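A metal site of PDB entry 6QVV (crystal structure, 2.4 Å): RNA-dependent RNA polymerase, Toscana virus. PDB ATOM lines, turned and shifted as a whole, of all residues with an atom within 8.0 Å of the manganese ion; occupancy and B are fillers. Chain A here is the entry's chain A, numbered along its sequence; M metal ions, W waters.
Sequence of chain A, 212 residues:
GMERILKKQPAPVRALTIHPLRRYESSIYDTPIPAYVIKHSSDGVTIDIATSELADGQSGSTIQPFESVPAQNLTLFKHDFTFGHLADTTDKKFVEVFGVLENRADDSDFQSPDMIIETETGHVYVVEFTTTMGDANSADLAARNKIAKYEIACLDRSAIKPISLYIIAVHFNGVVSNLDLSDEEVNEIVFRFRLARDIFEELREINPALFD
O of Val 127 lies within hydrogen-bond range of N of Asp 114.
The side-chain carboxylate (OE2) of Glu 128 sits close to the side-chain amino group (NZ) of Lys 146 (3.9 Å).
The backbone NH (N) of Ile 168 is in hydrogen-bond range of the backbone carbonyl oxygen (O) of Glu 128, at 3.0 Å.
OD1 of Asp 80 lies within hydrogen-bond range of ND1 of His 79 (2.6 Å).
Of the 16 residues printed, 4 come within 4 Å of the manganese ion.
The nearest printed residue that does not touch the manganese ion is Thr 130 (4.4 Å).
The manganese ion is bound by the backbone carbonyl oxygen (O) of Phe 129 (2.3 Å), the side-chain carboxylate (OD2) of Asp 114 (2.3 Å), water W2 (2.4 Å), the side-chain carboxylate (OE2) of Glu 128 (2.4 Å), a ring nitrogen (NE2) of His 79 (2.5 Å) and water W1 (2.5 Å).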
ATOM      1  N   HIS A  79      -4.595  -8.991  19.238  1.00  0.00           N
ATOM      2  CA  HIS A  79      -4.518 -10.396  19.634  1.00  0.00           C
ATOM      3  C   HIS A  79      -3.123 -10.751  20.143  1.00  0.00           C
ATOM      4  O   HIS A  79      -2.987 -11.380  21.197  1.00  0.00           O
ATOM      5  CB  HIS A  79      -4.924 -11.238  18.420  1.00  0.00           C
ATOM      6  CG  HIS A  79      -4.560 -12.678  18.500  1.00  0.00           C
ATOM      7  ND1 HIS A  79      -3.273 -13.139  18.287  1.00  0.00           N
ATOM      8  CD2 HIS A  79      -5.323 -13.785  18.693  1.00  0.00           C
ATOM      9  CE1 HIS A  79      -3.261 -14.458  18.392  1.00  0.00           C
ATOM     10  NE2 HIS A  79      -4.486 -14.868  18.640  1.00  0.00           N
ATOM     11  N   ASP A  80      -2.077 -10.312  19.446  1.00  0.00           N
ATOM     12  CA  ASP A  80      -0.730 -10.735  19.800  1.00  0.00           C
ATOM     13  C   ASP A  80      -0.227 -10.061  21.072  1.00  0.00           C
ATOM     14  O   ASP A  80       0.427 -10.698  21.908  1.00  0.00           O
ATOM     15  CB  ASP A  80       0.210 -10.474  18.618  1.00  0.00           C
ATOM     16  CG  ASP A  80       0.029 -11.496  17.483  1.00  0.00           C
ATOM     17  OD1 ASP A  80      -0.888 -12.352  17.569  1.00  0.00           O
ATOM     18  OD2 ASP A  80       0.798 -11.435  16.503  1.00  0.00           O
ATOM     19  N   PHE A  83      -1.909 -11.645  24.318  1.00  0.00           N
ATOM     20  CA  PHE A  83      -1.494 -12.990  24.698  1.00  0.00           C
ATOM     21  C   PHE A  83       0.023 -13.146  24.691  1.00  0.00           C
ATOM     22  O   PHE A  83       0.514 -14.280  24.822  1.00  0.00           O
ATOM     23  CB  PHE A  83      -2.168 -14.024  23.788  1.00  0.00           C
ATOM     24  CG  PHE A  83      -3.661 -14.070  23.943  1.00  0.00           C
ATOM     25  CD1 PHE A  83      -4.247 -14.659  25.056  1.00  0.00           C
ATOM     26  CD2 PHE A  83      -4.498 -13.486  22.989  1.00  0.00           C
ATOM     27  CE1 PHE A  83      -5.639 -14.674  25.231  1.00  0.00           C
ATOM     28  CE2 PHE A  83      -5.885 -13.512  23.149  1.00  0.00           C
ATOM     29  CZ  PHE A  83      -6.461 -14.115  24.274  1.00  0.00           C
ATOM     30  N   SER A 112      -2.914 -23.355  11.443  1.00  0.00           N
ATOM     31  CA  SER A 112      -1.897 -22.951  12.415  1.00  0.00           C
ATOM     32  C   SER A 112      -2.546 -22.359  13.666  1.00  0.00           C
ATOM     33  O   SER A 112      -2.729 -21.143  13.770  1.00  0.00           O
ATOM     34  CB  SER A 112      -0.926 -21.947  11.792  1.00  0.00           C
ATOM     35  OG  SER A 112       0.215 -21.759  12.613  1.00  0.00           O
ATOM     36  N   PRO A 113      -2.891 -23.204  14.627  1.00  0.00           N
ATOM     37  CA  PRO A 113      -3.421 -22.687  15.903  1.00  0.00           C
ATOM     38  C   PRO A 113      -2.306 -21.970  16.637  1.00  0.00           C
ATOM     39  O   PRO A 113      -1.128 -22.102  16.300  1.00  0.00           O
ATOM     40  CB  PRO A 113      -3.861 -23.946  16.635  1.00  0.00           C
ATOM     41  CG  PRO A 113      -2.963 -25.013  16.113  1.00  0.00           C
ATOM     42  CD  PRO A 113      -2.675 -24.658  14.674  1.00  0.00           C
ATOM     43  N   ASP A 114      -2.680 -21.197  17.668  1.00  0.00           N
ATOM     44  CA  ASP A 114      -1.683 -20.342  18.309  1.00  0.00           C
ATOM     45  C   ASP A 114      -0.596 -21.163  18.988  1.00  0.00           C
ATOM     46  O   ASP A 114       0.542 -20.691  19.096  1.00  0.00           O
ATOM     47  CB  ASP A 114      -2.341 -19.399  19.314  1.00  0.00           C
ATOM     48  CG  ASP A 114      -3.057 -18.256  18.646  1.00  0.00           C
ATOM     49  OD1 ASP A 114      -2.485 -17.620  17.748  1.00  0.00           O
ATOM     50  OD2 ASP A 114      -4.217 -17.998  18.989  1.00  0.00           O
ATOM     51  N   MET A 115      -0.914 -22.365  19.465  1.00  0.00           N
ATOM     52  CA  MET A 115       0.101 -23.244  20.037  1.00  0.00           C
ATOM     53  C   MET A 115      -0.233 -24.683  19.710  1.00  0.00           C
ATOM     54  O   MET A 115      -1.404 -25.082  19.691  1.00  0.00           O
ATOM     55  CB  MET A 115       0.220 -23.091  21.545  1.00  0.00           C
ATOM     56  CG  MET A 115       0.182 -21.665  22.034  1.00  0.00           C
ATOM     57  SD  MET A 115       0.324 -21.647  23.830  1.00  0.00           S
ATOM     58  CE  MET A 115       2.064 -22.004  23.979  1.00  0.00           C
ATOM     59  N   VAL A 127      -3.792 -25.100  21.479  1.00  0.00           N
ATOM     60  CA  VAL A 127      -4.247 -23.940  22.242  1.00  0.00           C
ATOM     61  C   VAL A 127      -4.497 -22.812  21.272  1.00  0.00           C
ATOM     62  O   VAL A 127      -3.646 -22.510  20.425  1.00  0.00           O
ATOM     63  CB  VAL A 127      -3.223 -23.525  23.322  1.00  0.00           C
ATOM     64  CG1 VAL A 127      -3.763 -22.370  24.214  1.00  0.00           C
ATOM     65  CG2 VAL A 127      -2.857 -24.712  24.167  1.00  0.00           C
ATOM     66  N   GLU A 128      -5.661 -22.192  21.361  1.00  0.00           N
ATOM     67  CA  GLU A 128      -6.025 -21.117  20.457  1.00  0.00           C
ATOM     68  C   GLU A 128      -6.522 -19.933  21.280  1.00  0.00           C
ATOM     69  O   GLU A 128      -7.309 -20.111  22.211  1.00  0.00           O
ATOM     70  CB  GLU A 128      -7.090 -21.580  19.474  1.00  0.00           C
ATOM     71  CG  GLU A 128      -7.667 -20.468  18.645  1.00  0.00           C
ATOM     72  CD  GLU A 128      -6.661 -19.900  17.683  1.00  0.00           C
ATOM     73  OE1 GLU A 128      -5.606 -20.508  17.440  1.00  0.00           O
ATOM     74  OE2 GLU A 128      -6.942 -18.807  17.154  1.00  0.00           O
ATOM     75  N   PHE A 129      -6.046 -18.733  20.926  1.00  0.00           N
ATOM     76  CA  PHE A 129      -6.415 -17.499  21.601  1.00  0.00           C
ATOM     77  C   PHE A 129      -7.361 -16.702  20.717  1.00  0.00           C
ATOM     78  O   PHE A 129      -7.324 -16.820  19.495  1.00  0.00           O
ATOM     79  CB  PHE A 129      -5.186 -16.611  21.911  1.00  0.00           C
ATOM     80  CG  PHE A 129      -4.040 -17.342  22.557  1.00  0.00           C
ATOM     81  CD1 PHE A 129      -4.245 -18.154  23.662  1.00  0.00           C
ATOM     82  CD2 PHE A 129      -2.761 -17.206  22.065  1.00  0.00           C
ATOM     83  CE1 PHE A 129      -3.187 -18.828  24.255  1.00  0.00           C
ATOM     84  CE2 PHE A 129      -1.696 -17.874  22.643  1.00  0.00           C
ATOM     85  CZ  PHE A 129      -1.921 -18.696  23.736  1.00  0.00           C
ATOM     86  N   THR A 130      -8.200 -15.871  21.320  1.00  0.00           N
ATOM     87  CA  THR A 130      -9.044 -14.993  20.512  1.00  0.00           C
ATOM     88  C   THR A 130      -9.582 -13.898  21.421  1.00  0.00           C
ATOM     89  O   THR A 130      -9.404 -13.942  22.631  1.00  0.00           O
ATOM     90  CB  THR A 130     -10.160 -15.781  19.802  1.00  0.00           C
ATOM     91  OG1 THR A 130     -10.814 -14.935  18.858  1.00  0.00           O
ATOM     92  CG2 THR A 130     -11.180 -16.361  20.780  1.00  0.00           C
ATOM     93  N   THR A 131     -10.194 -12.899  20.797  1.00  0.00           N
ATOM     94  CA  THR A 131     -10.677 -11.708  21.481  1.00  0.00           C
ATOM     95  C   THR A 131     -12.033 -11.313  20.918  1.00  0.00           C
ATOM     96  O   THR A 131     -12.412 -11.728  19.816  1.00  0.00           O
ATOM     97  CB  THR A 131      -9.710 -10.504  21.319  1.00  0.00           C
ATOM     98  OG1 THR A 131     -10.025  -9.804  20.114  1.00  0.00           O
ATOM     99  CG2 THR A 131      -8.247 -10.944  21.293  1.00  0.00           C
ATOM    100  N   LYS A 146     -13.802 -20.826  17.580  1.00  0.00           N
ATOM    101  CA  LYS A 146     -12.458 -21.366  17.438  1.00  0.00           C
ATOM    102  C   LYS A 146     -12.461 -22.888  17.567  1.00  0.00           C
ATOM    103  O   LYS A 146     -11.708 -23.578  16.866  1.00  0.00           O
ATOM    104  CB  LYS A 146     -11.505 -20.746  18.479  1.00  0.00           C
ATOM    105  CG  LYS A 146     -11.150 -19.314  18.191  1.00  0.00           C
ATOM    106  CD  LYS A 146     -10.749 -19.090  16.738  1.00  0.00           C
ATOM    107  CE  LYS A 146     -10.320 -17.628  16.527  1.00  0.00           C
ATOM    108  NZ  LYS A 146      -9.902 -17.368  15.116  1.00  0.00           N
ATOM    109  N   LYS A 149     -13.549 -24.099  14.277  1.00  0.00           N
ATOM    110  CA  LYS A 149     -12.477 -23.918  13.291  1.00  0.00           C
ATOM    111  C   LYS A 149     -11.471 -25.071  13.312  1.00  0.00           C
ATOM    112  O   LYS A 149     -10.991 -25.498  12.259  1.00  0.00           O
ATOM    113  CB  LYS A 149     -11.775 -22.580  13.534  1.00  0.00           C
ATOM    114  CG  LYS A 149     -10.564 -22.322  12.623  1.00  0.00           C
ATOM    115  CD  LYS A 149     -10.061 -20.888  12.778  1.00  0.00           C
ATOM    116  CE  LYS A 149      -8.935 -20.578  11.806  1.00  0.00           C
ATOM    117  NZ  LYS A 149      -9.447 -20.266  10.448  1.00  0.00           N
ATOM    118  N   TYR A 150     -11.152 -25.607  14.492  1.00  0.00           N
ATOM    119  CA  TYR A 150     -10.044 -26.559  14.604  1.00  0.00           C
ATOM    120  C   TYR A 150     -10.432 -27.972  15.007  1.00  0.00           C
ATOM    121  O   TYR A 150      -9.553 -28.836  15.027  1.00  0.00           O
ATOM    122  CB  TYR A 150      -9.001 -26.037  15.602  1.00  0.00           C
ATOM    123  CG  TYR A 150      -8.299 -24.792  15.120  1.00  0.00           C
ATOM    124  CD1 TYR A 150      -7.323 -24.858  14.139  1.00  0.00           C
ATOM    125  CD2 TYR A 150      -8.639 -23.539  15.641  1.00  0.00           C
ATOM    126  CE1 TYR A 150      -6.677 -23.726  13.695  1.00  0.00           C
ATOM    127  CE2 TYR A 150      -8.017 -22.406  15.201  1.00  0.00           C
ATOM    128  CZ  TYR A 150      -7.022 -22.503  14.222  1.00  0.00           C
ATOM    129  OH  TYR A 150      -6.380 -21.364  13.771  1.00  0.00           O
ATOM    130  N   ILE A 168      -8.718 -19.802  24.850  1.00  0.00           N
ATOM    131  CA  ILE A 168      -8.829 -18.611  25.694  1.00  0.00           C
ATOM    132  C   ILE A 168      -9.491 -17.533  24.862  1.00  0.00           C
ATOM    133  O   ILE A 168      -8.952 -17.124  23.823  1.00  0.00           O
ATOM    134  CB  ILE A 168      -7.465 -18.135  26.217  1.00  0.00           C
ATOM    135  CG1 ILE A 168      -6.683 -19.267  26.896  1.00  0.00           C
ATOM    136  CG2 ILE A 168      -7.639 -17.035  27.231  1.00  0.00           C
ATOM    137  CD1 ILE A 168      -5.260 -18.848  27.327  1.00  0.00           C
HETATM  138 MN    MN M   1      -5.782 -16.788  17.786  1.00  0.00          MN
HETATM  139  O   HOH W   1      -7.361 -15.617  16.180  1.00  0.00           O
HETATM  140  O   HOH W   2      -4.225 -17.253  16.039  1.00  0.00           O
